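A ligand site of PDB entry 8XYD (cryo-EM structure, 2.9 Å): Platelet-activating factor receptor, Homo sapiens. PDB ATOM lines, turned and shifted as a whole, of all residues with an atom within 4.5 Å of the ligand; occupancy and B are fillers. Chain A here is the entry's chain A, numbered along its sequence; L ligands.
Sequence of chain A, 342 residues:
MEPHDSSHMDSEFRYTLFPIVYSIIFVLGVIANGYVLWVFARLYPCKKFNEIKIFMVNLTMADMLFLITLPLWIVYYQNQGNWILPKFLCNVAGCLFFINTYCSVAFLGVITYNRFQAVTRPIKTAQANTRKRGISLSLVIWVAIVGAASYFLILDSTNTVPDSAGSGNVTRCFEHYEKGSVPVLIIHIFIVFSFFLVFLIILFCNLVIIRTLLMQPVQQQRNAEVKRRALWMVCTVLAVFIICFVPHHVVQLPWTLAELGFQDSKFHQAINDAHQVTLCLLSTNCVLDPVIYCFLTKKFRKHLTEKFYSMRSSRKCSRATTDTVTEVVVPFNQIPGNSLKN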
ATOM      1  N   TYR A  22     -35.600  16.433 -21.973  1.00  0.00           N
ATOM      2  CA  TYR A  22     -34.295  16.568 -21.330  1.00  0.00           C
ATOM      3  C   TYR A  22     -33.704  17.967 -21.549  1.00  0.00           C
ATOM      4  O   TYR A  22     -33.077  18.508 -20.655  1.00  0.00           O
ATOM      5  CB  TYR A  22     -33.327  15.494 -21.843  1.00  0.00           C
ATOM      6  CG  TYR A  22     -33.179  14.231 -21.025  1.00  0.00           C
ATOM      7  CD1 TYR A  22     -33.094  14.264 -19.639  1.00  0.00           C
ATOM      8  CD2 TYR A  22     -33.126  12.979 -21.639  1.00  0.00           C
ATOM      9  CE1 TYR A  22     -32.972  13.096 -18.898  1.00  0.00           C
ATOM     10  CE2 TYR A  22     -32.994  11.811 -20.909  1.00  0.00           C
ATOM     11  CZ  TYR A  22     -32.899  11.870 -19.531  1.00  0.00           C
ATOM     12  OH  TYR A  22     -32.781  10.718 -18.793  1.00  0.00           O
ATOM     13  N   TRP A  73     -26.546  12.584 -23.171  1.00  0.00           N
ATOM     14  CA  TRP A  73     -27.611  11.640 -23.476  1.00  0.00           C
ATOM     15  C   TRP A  73     -28.659  12.245 -24.387  1.00  0.00           C
ATOM     16  O   TRP A  73     -29.300  11.528 -25.160  1.00  0.00           O
ATOM     17  CB  TRP A  73     -28.257  11.152 -22.176  1.00  0.00           C
ATOM     18  CG  TRP A  73     -27.338  10.344 -21.326  1.00  0.00           C
ATOM     19  CD1 TRP A  73     -26.651  10.774 -20.224  1.00  0.00           C
ATOM     20  CD2 TRP A  73     -26.979   8.969 -21.515  1.00  0.00           C
ATOM     21  NE1 TRP A  73     -25.900   9.742 -19.712  1.00  0.00           N
ATOM     22  CE2 TRP A  73     -26.086   8.629 -20.488  1.00  0.00           C
ATOM     23  CE3 TRP A  73     -27.345   7.999 -22.445  1.00  0.00           C
ATOM     24  CZ2 TRP A  73     -25.539   7.353 -20.359  1.00  0.00           C
ATOM     25  CZ3 TRP A  73     -26.797   6.729 -22.325  1.00  0.00           C
ATOM     26  CH2 TRP A  73     -25.913   6.417 -21.295  1.00  0.00           C
ATOM     27  N   TYR A  77     -29.850  10.210 -27.674  1.00  0.00           N
ATOM     28  CA  TYR A  77     -31.235   9.901 -28.053  1.00  0.00           C
ATOM     29  C   TYR A  77     -31.661  10.618 -29.320  1.00  0.00           C
ATOM     30  O   TYR A  77     -32.531  10.116 -30.043  1.00  0.00           O
ATOM     31  CB  TYR A  77     -32.186  10.263 -26.907  1.00  0.00           C
ATOM     32  CG  TYR A  77     -32.007   9.391 -25.675  1.00  0.00           C
ATOM     33  CD1 TYR A  77     -31.558   9.927 -24.480  1.00  0.00           C
ATOM     34  CD2 TYR A  77     -32.284   8.025 -25.730  1.00  0.00           C
ATOM     35  CE1 TYR A  77     -31.398   9.127 -23.359  1.00  0.00           C
ATOM     36  CE2 TYR A  77     -32.122   7.230 -24.618  1.00  0.00           C
ATOM     37  CZ  TYR A  77     -31.681   7.779 -23.439  1.00  0.00           C
ATOM     38  OH  TYR A  77     -31.520   6.984 -22.327  1.00  0.00           O
ATOM     39  N   PHE A  97     -24.396  10.075 -14.305  1.00  0.00           N
ATOM     40  CA  PHE A  97     -25.848  10.077 -14.173  1.00  0.00           C
ATOM     41  C   PHE A  97     -26.310   9.388 -12.908  1.00  0.00           C
ATOM     42  O   PHE A  97     -27.069   9.964 -12.131  1.00  0.00           O
ATOM     43  CB  PHE A  97     -26.398   9.307 -15.376  1.00  0.00           C
ATOM     44  CG  PHE A  97     -27.861   9.523 -15.653  1.00  0.00           C
ATOM     45  CD1 PHE A  97     -28.256  10.437 -16.608  1.00  0.00           C
ATOM     46  CD2 PHE A  97     -28.828   8.768 -15.009  1.00  0.00           C
ATOM     47  CE1 PHE A  97     -29.598  10.630 -16.888  1.00  0.00           C
ATOM     48  CE2 PHE A  97     -30.170   8.956 -15.280  1.00  0.00           C
ATOM     49  CZ  PHE A  97     -30.557   9.885 -16.226  1.00  0.00           C
ATOM     50  N   PHE A  98     -25.861   8.159 -12.683  1.00  0.00           N
ATOM     51  CA  PHE A  98     -26.308   7.373 -11.548  1.00  0.00           C
ATOM     52  C   PHE A  98     -25.738   7.894 -10.237  1.00  0.00           C
ATOM     53  O   PHE A  98     -26.465   7.985  -9.238  1.00  0.00           O
ATOM     54  CB  PHE A  98     -25.925   5.904 -11.751  1.00  0.00           C
ATOM     55  CG  PHE A  98     -26.784   5.192 -12.755  1.00  0.00           C
ATOM     56  CD1 PHE A  98     -27.635   4.176 -12.354  1.00  0.00           C
ATOM     57  CD2 PHE A  98     -26.745   5.533 -14.091  1.00  0.00           C
ATOM     58  CE1 PHE A  98     -28.430   3.507 -13.272  1.00  0.00           C
ATOM     59  CE2 PHE A  98     -27.544   4.882 -15.013  1.00  0.00           C
ATOM     60  CZ  PHE A  98     -28.381   3.869 -14.609  1.00  0.00           C
ATOM     61  N   TYR A 102     -28.212   9.148  -7.256  1.00  0.00           N
ATOM     62  CA  TYR A 102     -28.257   8.435  -5.992  1.00  0.00           C
ATOM     63  C   TYR A 102     -27.610   9.158  -4.817  1.00  0.00           C
ATOM     64  O   TYR A 102     -27.934   8.884  -3.673  1.00  0.00           O
ATOM     65  CB  TYR A 102     -27.766   6.997  -6.147  1.00  0.00           C
ATOM     66  CG  TYR A 102     -28.695   6.222  -7.065  1.00  0.00           C
ATOM     67  CD1 TYR A 102     -30.060   6.218  -6.850  1.00  0.00           C
ATOM     68  CD2 TYR A 102     -28.201   5.520  -8.157  1.00  0.00           C
ATOM     69  CE1 TYR A 102     -30.916   5.532  -7.681  1.00  0.00           C
ATOM     70  CE2 TYR A 102     -29.056   4.838  -8.997  1.00  0.00           C
ATOM     71  CZ  TYR A 102     -30.414   4.842  -8.755  1.00  0.00           C
ATOM     72  OH  TYR A 102     -31.261   4.151  -9.588  1.00  0.00           O
ATOM     73  N   VAL A 105     -30.336  11.545  -3.809  1.00  0.00           N
ATOM     74  CA  VAL A 105     -31.317  10.847  -2.988  1.00  0.00           C
ATOM     75  C   VAL A 105     -30.809  10.702  -1.559  1.00  0.00           C
ATOM     76  O   VAL A 105     -31.555  10.934  -0.590  1.00  0.00           O
ATOM     77  CB  VAL A 105     -31.650   9.464  -3.601  1.00  0.00           C
ATOM     78  CG1 VAL A 105     -32.477   8.640  -2.631  1.00  0.00           C
ATOM     79  CG2 VAL A 105     -32.383   9.637  -4.920  1.00  0.00           C
ATOM     80  N   ALA A 106     -29.537  10.331  -1.391  1.00  0.00           N
ATOM     81  CA  ALA A 106     -28.985  10.168  -0.059  1.00  0.00           C
ATOM     82  C   ALA A 106     -28.942  11.494   0.693  1.00  0.00           C
ATOM     83  O   ALA A 106     -29.206  11.539   1.910  1.00  0.00           O
ATOM     84  CB  ALA A 106     -27.579   9.558  -0.143  1.00  0.00           C
ATOM     85  N   ILE A 145     -20.070   6.040  -3.267  1.00  0.00           N
ATOM     86  CA  ILE A 145     -20.737   6.028  -4.565  1.00  0.00           C
ATOM     87  C   ILE A 145     -19.695   5.997  -5.688  1.00  0.00           C
ATOM     88  O   ILE A 145     -19.873   5.283  -6.682  1.00  0.00           O
ATOM     89  CB  ILE A 145     -21.674   7.238  -4.692  1.00  0.00           C
ATOM     90  CG1 ILE A 145     -22.814   7.127  -3.675  1.00  0.00           C
ATOM     91  CG2 ILE A 145     -22.233   7.336  -6.104  1.00  0.00           C
ATOM     92  CD1 ILE A 145     -23.686   8.359  -3.569  1.00  0.00           C
ATOM     93  N   ALA A 148     -18.308   2.512  -5.935  1.00  0.00           N
ATOM     94  CA  ALA A 148     -19.280   1.605  -6.541  1.00  0.00           C
ATOM     95  C   ALA A 148     -19.361   1.825  -8.043  1.00  0.00           C
ATOM     96  O   ALA A 148     -19.525   0.863  -8.816  1.00  0.00           O
ATOM     97  CB  ALA A 148     -20.646   1.787  -5.899  1.00  0.00           C
ATOM     98  N   ALA A 149     -19.253   3.075  -8.495  1.00  0.00           N
ATOM     99  CA  ALA A 149     -19.354   3.371  -9.912  1.00  0.00           C
ATOM    100  C   ALA A 149     -18.069   3.093 -10.669  1.00  0.00           C
ATOM    101  O   ALA A 149     -18.113   2.924 -11.898  1.00  0.00           O
ATOM    102  CB  ALA A 149     -19.740   4.840 -10.106  1.00  0.00           C
ATOM    103  N   PHE A 152     -18.099  -0.202 -12.907  1.00  0.00           N
ATOM    104  CA  PHE A 152     -18.786  -0.039 -14.183  1.00  0.00           C
ATOM    105  C   PHE A 152     -18.130   1.018 -15.055  1.00  0.00           C
ATOM    106  O   PHE A 152     -18.383   1.045 -16.264  1.00  0.00           O
ATOM    107  CB  PHE A 152     -20.262   0.307 -13.949  1.00  0.00           C
ATOM    108  CG  PHE A 152     -21.070  -0.837 -13.408  1.00  0.00           C
ATOM    109  CD1 PHE A 152     -21.028  -1.169 -12.071  1.00  0.00           C
ATOM    110  CD2 PHE A 152     -21.879  -1.587 -14.258  1.00  0.00           C
ATOM    111  CE1 PHE A 152     -21.774  -2.227 -11.581  1.00  0.00           C
ATOM    112  CE2 PHE A 152     -22.624  -2.641 -13.777  1.00  0.00           C
ATOM    113  CZ  PHE A 152     -22.578  -2.965 -12.436  1.00  0.00           C
ATOM    114  N   PHE A 174     -24.205   2.069 -22.372  1.00  0.00           N
ATOM    115  CA  PHE A 174     -24.740   1.849 -21.023  1.00  0.00           C
ATOM    116  C   PHE A 174     -26.152   1.298 -20.954  1.00  0.00           C
ATOM    117  O   PHE A 174     -26.806   1.367 -19.915  1.00  0.00           O
ATOM    118  CB  PHE A 174     -24.637   3.128 -20.177  1.00  0.00           C
ATOM    119  CG  PHE A 174     -24.066   2.917 -18.800  1.00  0.00           C
ATOM    120  CD1 PHE A 174     -22.694   2.800 -18.614  1.00  0.00           C
ATOM    121  CD2 PHE A 174     -24.894   2.813 -17.698  1.00  0.00           C
ATOM    122  CE1 PHE A 174     -22.166   2.605 -17.358  1.00  0.00           C
ATOM    123  CE2 PHE A 174     -24.371   2.605 -16.438  1.00  0.00           C
ATOM    124  CZ  PHE A 174     -23.007   2.501 -16.268  1.00  0.00           C
ATOM    125  N   GLU A 175     -26.631   0.740 -22.061  1.00  0.00           N
ATOM    126  CA  GLU A 175     -27.968   0.167 -22.088  1.00  0.00           C
ATOM    127  C   GLU A 175     -28.002  -1.029 -23.009  1.00  0.00           C
ATOM    128  O   GLU A 175     -26.963  -1.417 -23.549  1.00  0.00           O
ATOM    129  CB  GLU A 175     -28.977   1.208 -22.583  1.00  0.00           C
ATOM    130  CG  GLU A 175     -28.742   1.676 -24.007  1.00  0.00           C
ATOM    131  CD  GLU A 175     -29.827   2.618 -24.504  1.00  0.00           C
ATOM    132  OE1 GLU A 175     -29.485   3.709 -24.998  1.00  0.00           O
ATOM    133  OE2 GLU A 175     -31.019   2.259 -24.394  1.00  0.00           O
ATOM    134  N   HIS A 176     -29.174  -1.627 -23.183  1.00  0.00           N
ATOM    135  CA  HIS A 176     -29.331  -2.760 -24.081  1.00  0.00           C
ATOM    136  C   HIS A 176     -28.193  -3.769 -24.001  1.00  0.00           C
ATOM    137  O   HIS A 176     -27.494  -4.004 -24.988  1.00  0.00           O
ATOM    138  CB  HIS A 176     -29.503  -2.287 -25.524  1.00  0.00           C
ATOM    139  CG  HIS A 176     -30.893  -1.815 -25.830  1.00  0.00           C
ATOM    140  ND1 HIS A 176     -31.541  -0.873 -25.065  1.00  0.00           N
ATOM    141  CD2 HIS A 176     -31.751  -2.143 -26.823  1.00  0.00           C
ATOM    142  CE1 HIS A 176     -32.748  -0.652 -25.558  1.00  0.00           C
ATOM    143  NE2 HIS A 176     -32.897  -1.427 -26.628  1.00  0.00           N
ATOM    144  N   TYR A 177     -28.011  -4.354 -22.832  1.00  0.00           N
ATOM    145  CA  TYR A 177     -26.940  -5.325 -22.647  1.00  0.00           C
ATOM    146  C   TYR A 177     -27.329  -6.670 -23.233  1.00  0.00           C
ATOM    147  O   TYR A 177     -28.511  -6.936 -23.471  1.00  0.00           O
ATOM    148  CB  TYR A 177     -26.606  -5.484 -21.172  1.00  0.00           C
ATOM    149  CG  TYR A 177     -26.097  -4.216 -20.514  1.00  0.00           C
ATOM    150  CD1 TYR A 177     -26.597  -3.802 -19.292  1.00  0.00           C
ATOM    151  CD2 TYR A 177     -25.116  -3.439 -21.123  1.00  0.00           C
ATOM    152  CE1 TYR A 177     -26.133  -2.646 -18.686  1.00  0.00           C
ATOM    153  CE2 TYR A 177     -24.656  -2.291 -20.522  1.00  0.00           C
ATOM    154  CZ  TYR A 177     -25.164  -1.892 -19.308  1.00  0.00           C
ATOM    155  OH  TYR A 177     -24.703  -0.745 -18.707  1.00  0.00           O
ATOM    156  N   VAL A 184     -24.477  -6.499 -13.308  1.00  0.00           N
ATOM    157  CA  VAL A 184     -25.540  -5.526 -13.526  1.00  0.00           C
ATOM    158  C   VAL A 184     -26.732  -5.817 -12.631  1.00  0.00           C
ATOM    159  O   VAL A 184     -27.280  -4.916 -11.971  1.00  0.00           O
ATOM    160  CB  VAL A 184     -25.954  -5.499 -15.009  1.00  0.00           C
ATOM    161  CG1 VAL A 184     -27.111  -4.539 -15.230  1.00  0.00           C
ATOM    162  CG2 VAL A 184     -24.761  -5.111 -15.875  1.00  0.00           C
ATOM    163  N   ILE A 187     -25.774  -4.855  -8.978  1.00  0.00           N
ATOM    164  CA  ILE A 187     -25.831  -3.426  -8.691  1.00  0.00           C
ATOM    165  C   ILE A 187     -27.266  -2.918  -8.732  1.00  0.00           C
ATOM    166  O   ILE A 187     -27.645  -2.113  -7.904  1.00  0.00           O
ATOM    167  CB  ILE A 187     -24.880  -2.593  -9.589  1.00  0.00           C
ATOM    168  CG1 ILE A 187     -24.879  -1.137  -9.135  1.00  0.00           C
ATOM    169  CG2 ILE A 187     -25.240  -2.677 -11.059  1.00  0.00           C
ATOM    170  CD1 ILE A 187     -23.764  -0.305  -9.738  1.00  0.00           C
ATOM    171  N   HIS A 188     -28.079  -3.423  -9.656  1.00  0.00           N
ATOM    172  CA  HIS A 188     -29.464  -2.984  -9.752  1.00  0.00           C
ATOM    173  C   HIS A 188     -30.176  -3.361  -8.478  1.00  0.00           C
ATOM    174  O   HIS A 188     -30.808  -2.516  -7.844  1.00  0.00           O
ATOM    175  CB  HIS A 188     -30.154  -3.591 -10.959  1.00  0.00           C
ATOM    176  CG  HIS A 188     -30.193  -2.688 -12.151  1.00  0.00           C
ATOM    177  ND1 HIS A 188     -29.063  -2.328 -12.844  1.00  0.00           N
ATOM    178  CD2 HIS A 188     -31.231  -2.061 -12.755  1.00  0.00           C
ATOM    179  CE1 HIS A 188     -29.396  -1.514 -13.836  1.00  0.00           C
ATOM    180  NE2 HIS A 188     -30.701  -1.341 -13.805  1.00  0.00           N
ATOM    181  N   PHE A 190     -28.879  -3.972  -5.620  1.00  0.00           N
ATOM    182  CA  PHE A 190     -28.315  -3.187  -4.522  1.00  0.00           C
ATOM    183  C   PHE A 190     -29.009  -1.836  -4.453  1.00  0.00           C
ATOM    184  O   PHE A 190     -29.487  -1.444  -3.387  1.00  0.00           O
ATOM    185  CB  PHE A 190     -26.810  -3.021  -4.708  1.00  0.00           C
ATOM    186  CG  PHE A 190     -26.215  -1.865  -3.956  1.00  0.00           C
ATOM    187  CD1 PHE A 190     -25.818  -0.717  -4.620  1.00  0.00           C
ATOM    188  CD2 PHE A 190     -26.043  -1.932  -2.582  1.00  0.00           C
ATOM    189  CE1 PHE A 190     -25.271   0.343  -3.922  1.00  0.00           C
ATOM    190  CE2 PHE A 190     -25.491  -0.884  -1.890  1.00  0.00           C
ATOM    191  CZ  PHE A 190     -25.108   0.260  -2.557  1.00  0.00           C
ATOM    192  N   ILE A 191     -29.076  -1.126  -5.568  1.00  0.00           N
ATOM    193  CA  ILE A 191     -29.693   0.184  -5.605  1.00  0.00           C
ATOM    194  C   ILE A 191     -31.136   0.095  -5.147  1.00  0.00           C
ATOM    195  O   ILE A 191     -31.568   0.835  -4.267  1.00  0.00           O
ATOM    196  CB  ILE A 191     -29.635   0.776  -7.023  1.00  0.00           C
ATOM    197  CG1 ILE A 191     -28.235   1.320  -7.312  1.00  0.00           C
ATOM    198  CG2 ILE A 191     -30.683   1.850  -7.209  1.00  0.00           C
ATOM    199  CD1 ILE A 191     -27.722   2.284  -6.260  1.00  0.00           C
ATOM    200  N   SER A 194     -31.189  -0.345  -1.355  1.00  0.00           N
ATOM    201  CA  SER A 194     -30.737   0.853  -0.660  1.00  0.00           C
ATOM    202  C   SER A 194     -31.760   1.959  -0.770  1.00  0.00           C
ATOM    203  O   SER A 194     -32.126   2.577   0.243  1.00  0.00           O
ATOM    204  CB  SER A 194     -29.407   1.329  -1.229  1.00  0.00           C
ATOM    205  OG  SER A 194     -28.484   0.260  -1.312  1.00  0.00           O
ATOM    206  N   PHE A 195     -32.225   2.234  -1.979  1.00  0.00           N
ATOM    207  CA  PHE A 195     -33.224   3.271  -2.169  1.00  0.00           C
ATOM    208  C   PHE A 195     -34.431   3.002  -1.298  1.00  0.00           C
ATOM    209  O   PHE A 195     -34.905   3.894  -0.625  1.00  0.00           O
ATOM    210  CB  PHE A 195     -33.690   3.369  -3.619  1.00  0.00           C
ATOM    211  CG  PHE A 195     -34.989   4.108  -3.787  1.00  0.00           C
ATOM    212  CD1 PHE A 195     -36.167   3.426  -4.052  1.00  0.00           C
ATOM    213  CD2 PHE A 195     -35.024   5.490  -3.659  1.00  0.00           C
ATOM    214  CE1 PHE A 195     -37.356   4.107  -4.197  1.00  0.00           C
ATOM    215  CE2 PHE A 195     -36.223   6.170  -3.793  1.00  0.00           C
ATOM    216  CZ  PHE A 195     -37.383   5.481  -4.061  1.00  0.00           C
ATOM    217  N   VAL A 198     -33.758   3.790   2.341  1.00  0.00           N
ATOM    218  CA  VAL A 198     -33.733   5.233   2.553  1.00  0.00           C
ATOM    219  C   VAL A 198     -35.135   5.838   2.532  1.00  0.00           C
ATOM    220  O   VAL A 198     -35.458   6.698   3.347  1.00  0.00           O
ATOM    221  CB  VAL A 198     -32.836   5.941   1.503  1.00  0.00           C
ATOM    222  CG1 VAL A 198     -32.869   7.444   1.662  1.00  0.00           C
ATOM    223  CG2 VAL A 198     -31.408   5.439   1.627  1.00  0.00           C
ATOM    224  N   HIS A 248     -39.876   4.643 -10.543  1.00  0.00           N
ATOM    225  CA  HIS A 248     -38.616   4.199 -11.140  1.00  0.00           C
ATOM    226  C   HIS A 248     -38.222   2.882 -10.581  1.00  0.00           C
ATOM    227  O   HIS A 248     -38.026   1.954 -11.318  1.00  0.00           O
ATOM    228  CB  HIS A 248     -37.485   5.159 -10.879  1.00  0.00           C
ATOM    229  CG  HIS A 248     -36.189   4.720 -11.471  1.00  0.00           C
ATOM    230  ND1 HIS A 248     -36.044   4.440 -12.811  1.00  0.00           N
ATOM    231  CD2 HIS A 248     -34.975   4.519 -10.911  1.00  0.00           C
ATOM    232  CE1 HIS A 248     -34.797   4.076 -13.049  1.00  0.00           C
ATOM    233  NE2 HIS A 248     -34.126   4.127 -11.912  1.00  0.00           N
ATOM    234  N   GLN A 252     -37.970  -0.412 -12.545  1.00  0.00           N
ATOM    235  CA  GLN A 252     -36.554  -0.723 -12.765  1.00  0.00           C
ATOM    236  C   GLN A 252     -36.176  -2.199 -12.597  1.00  0.00           C
ATOM    237  O   GLN A 252     -35.689  -2.815 -13.543  1.00  0.00           O
ATOM    238  CB  GLN A 252     -35.638   0.103 -11.855  1.00  0.00           C
ATOM    239  CG  GLN A 252     -34.270   0.396 -12.450  1.00  0.00           C
ATOM    240  CD  GLN A 252     -33.283   0.882 -11.407  1.00  0.00           C
ATOM    241  OE1 GLN A 252     -33.523   0.756 -10.200  1.00  0.00           O
ATOM    242  NE2 GLN A 252     -32.171   1.451 -11.855  1.00  0.00           N
ATOM    243  N   TRP A 255     -37.875  -4.616 -14.938  1.00  0.00           N
ATOM    244  CA  TRP A 255     -37.374  -4.469 -16.305  1.00  0.00           C
ATOM    245  C   TRP A 255     -35.991  -5.084 -16.450  1.00  0.00           C
ATOM    246  O   TRP A 255     -35.703  -5.765 -17.435  1.00  0.00           O
ATOM    247  CB  TRP A 255     -37.339  -2.969 -16.642  1.00  0.00           C
ATOM    248  CG  TRP A 255     -36.440  -2.544 -17.751  1.00  0.00           C
ATOM    249  CD1 TRP A 255     -36.732  -2.518 -19.077  1.00  0.00           C
ATOM    250  CD2 TRP A 255     -35.098  -2.049 -17.616  1.00  0.00           C
ATOM    251  NE1 TRP A 255     -35.656  -2.043 -19.792  1.00  0.00           N
ATOM    252  CE2 TRP A 255     -34.644  -1.751 -18.919  1.00  0.00           C
ATOM    253  CE3 TRP A 255     -34.243  -1.833 -16.535  1.00  0.00           C
ATOM    254  CZ2 TRP A 255     -33.366  -1.252 -19.151  1.00  0.00           C
ATOM    255  CZ3 TRP A 255     -32.978  -1.338 -16.771  1.00  0.00           C
ATOM    256  CH2 TRP A 255     -32.551  -1.053 -18.071  1.00  0.00           C
ATOM    257  N   HIS A 275     -41.081   2.042 -17.832  1.00  0.00           N
ATOM    258  CA  HIS A 275     -39.732   2.428 -17.403  1.00  0.00           C
ATOM    259  C   HIS A 275     -39.211   3.712 -18.064  1.00  0.00           C
ATOM    260  O   HIS A 275     -38.316   4.366 -17.541  1.00  0.00           O
ATOM    261  CB  HIS A 275     -38.753   1.269 -17.665  1.00  0.00           C
ATOM    262  CG  HIS A 275     -37.371   1.498 -17.147  1.00  0.00           C
ATOM    263  ND1 HIS A 275     -37.103   1.721 -15.815  1.00  0.00           N
ATOM    264  CD2 HIS A 275     -36.178   1.527 -17.783  1.00  0.00           C
ATOM    265  CE1 HIS A 275     -35.802   1.883 -15.656  1.00  0.00           C
ATOM    266  NE2 HIS A 275     -35.217   1.778 -16.834  1.00  0.00           N
ATOM    267  N   LEU A 279     -37.781   7.514 -15.851  1.00  0.00           N
ATOM    268  CA  LEU A 279     -36.553   8.291 -15.974  1.00  0.00           C
ATOM    269  C   LEU A 279     -36.982   9.727 -16.291  1.00  0.00           C
ATOM    270  O   LEU A 279     -36.349  10.729 -15.810  1.00  0.00           O
ATOM    271  CB  LEU A 279     -35.722   7.757 -17.131  1.00  0.00           C
ATOM    272  CG  LEU A 279     -35.151   6.340 -17.019  1.00  0.00           C
ATOM    273  CD1 LEU A 279     -34.474   5.928 -18.317  1.00  0.00           C
ATOM    274  CD2 LEU A 279     -34.194   6.248 -15.843  1.00  0.00           C
HETATM  275  C1  LIG L   1     -27.011  -0.448 -16.207  1.00  0.00           C
HETATM  276  O1  LIG L   1     -26.916   0.393 -15.095  1.00  0.00           O
HETATM  277  C2  LIG L   1     -28.221  -0.148 -17.101  1.00  0.00           C
HETATM  278  O2  LIG L   1     -29.214  -1.106 -16.873  1.00  0.00           O
HETATM  279  C3  LIG L   1     -29.396  -2.091 -17.853  1.00  0.00           C
HETATM  280  O3  LIG L   1     -29.532  -3.211 -17.516  1.00  0.00           O
HETATM  281  C4  LIG L   1     -29.466  -1.725 -19.333  1.00  0.00           C
HETATM  282  C5  LIG L   1     -28.839   1.206 -16.819  1.00  0.00           C
HETATM  283  C6  LIG L   1     -25.943  -0.073 -14.207  1.00  0.00           C
HETATM  284  C7  LIG L   1     -25.760   0.935 -13.068  1.00  0.00           C
HETATM  285  O4  LIG L   1     -30.198   1.020 -16.552  1.00  0.00           O
HETATM  286  P1  LIG L   1     -31.186   2.265 -16.983  1.00  0.00           P
HETATM  287  O5  LIG L   1     -31.944   2.777 -15.786  1.00  0.00           O
HETATM  288  O6  LIG L   1     -32.137   1.857 -18.083  1.00  0.00           O
HETATM  289  O7  LIG L   1     -30.202   3.432 -17.589  1.00  0.00           O
HETATM  290  C8  LIG L   1     -30.620   4.124 -18.731  1.00  0.00           C
HETATM  291  C9  LIG L   1     -30.641   5.593 -18.305  1.00  0.00           C
HETATM  292  N1  LIG L   1     -29.595   6.281 -19.035  1.00  0.00           N
HETATM  293  C10 LIG L   1     -30.028   7.618 -19.394  1.00  0.00           C
HETATM  294  C11 LIG L   1     -28.408   6.387 -18.212  1.00  0.00           C
HETATM  295  C12 LIG L   1     -29.322   5.472 -20.202  1.00  0.00           C
HETATM  296  C13 LIG L   1     -24.303   1.341 -12.858  1.00  0.00           C
HETATM  297  C14 LIG L   1     -24.151   2.789 -12.395  1.00  0.00           C
HETATM  298  C15 LIG L   1     -23.575   2.990 -10.993  1.00  0.00           C
HETATM  299  C16 LIG L   1     -24.597   3.027  -9.832  1.00  0.00           C
HETATM  300  C17 LIG L   1     -23.922   3.596  -8.612  1.00  0.00           C
HETATM  301  C18 LIG L   1     -24.479   2.905  -7.389  1.00  0.00           C
HETATM  302  C19 LIG L   1     -24.644   3.961  -6.287  1.00  0.00           C
HETATM  303  C20 LIG L   1     -25.093   3.315  -4.976  1.00  0.00           C
HETATM  304  C21 LIG L   1     -26.095   4.028  -4.089  1.00  0.00           C
HETATM  305  C22 LIG L   1     -26.997   3.159  -3.194  1.00  0.00           C
HETATM  306  C23 LIG L   1     -27.812   4.313  -2.694  1.00  0.00           C
HETATM  307  C24 LIG L   1     -29.220   4.519  -3.245  1.00  0.00           C
HETATM  308  C25 LIG L   1     -29.922   5.645  -2.489  1.00  0.00           C
HETATM  309  C26 LIG L   1     -29.249   6.073  -1.174  1.00  0.00           C
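OH of Tyr 177 lies within hydrogen-bond range of O of Phe 174 (3.2 Å). The backbone carbonyl oxygen (O) of Phe 190 lies within hydrogen-bond range of the side-chain hydroxyl (OG) of Ser 194 (2.9 Å). ND1 of His 188 lies within hydrogen-bond range of O of Val 184 (3.3 Å). ND1 of His 176 sits at hydrogen-bond distance from OE2 of Glu 175.
An oxygen (O6) of the ligand sits at hydrogen-bond distance from a ring nitrogen (NE2) of His 275, at 3.3 Å. A ring nitrogen (NE2) of His 188 lies close to an oxygen (O2) of the ligand (3.4 Å).
Merely in contact with the ligand: Trp 73 (3.5 Å), Tyr 77 (3.4 Å), Phe 97 (3.9 Å), Phe 98 (3.5 Å), Tyr 102 (3.98 Å), Val 105 (3.9 Å), Ala 106 (3.9996 Å), Phe 152 (3.9 Å), Phe 174 (3.5 Å), Glu 175 (3.7 Å), His 176 (3.9 Å), Tyr 177 (3.4 Å), Val 184 (3.6 Å), Ile 187 (3.4 Å), Phe 190 (3.2 Å), Ile 191 (3.1 Å), Ser 194 (3.6 Å), Phe 195 (3.98 Å), Val 198 (3.6 Å), Trp 255 (2.9 Å) and Leu 279 (3.8 Å). Hydrophobic or aromatic side chains that line the ligand: Trp 73, Phe 97, Phe 98, Tyr 102, Val 105, Ala 106, Phe 152, Phe 174, Tyr 177, Val 184, Ile 187, His 188, Phe 190, Ile 191, Val 198, Trp 255, His 275 and Leu 279. Within 4 Å of the ligand: Trp 73, Tyr 77, Phe 97, Phe 98, Tyr 102, Val 105, Ala 106, Phe 152, Phe 174, Glu 175, His 176, Tyr 177, Val 184, Ile 187, His 188, Phe 190, Ile 191, Ser 194, Phe 195, Val 198, Trp 255, His 275 and Leu 279.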
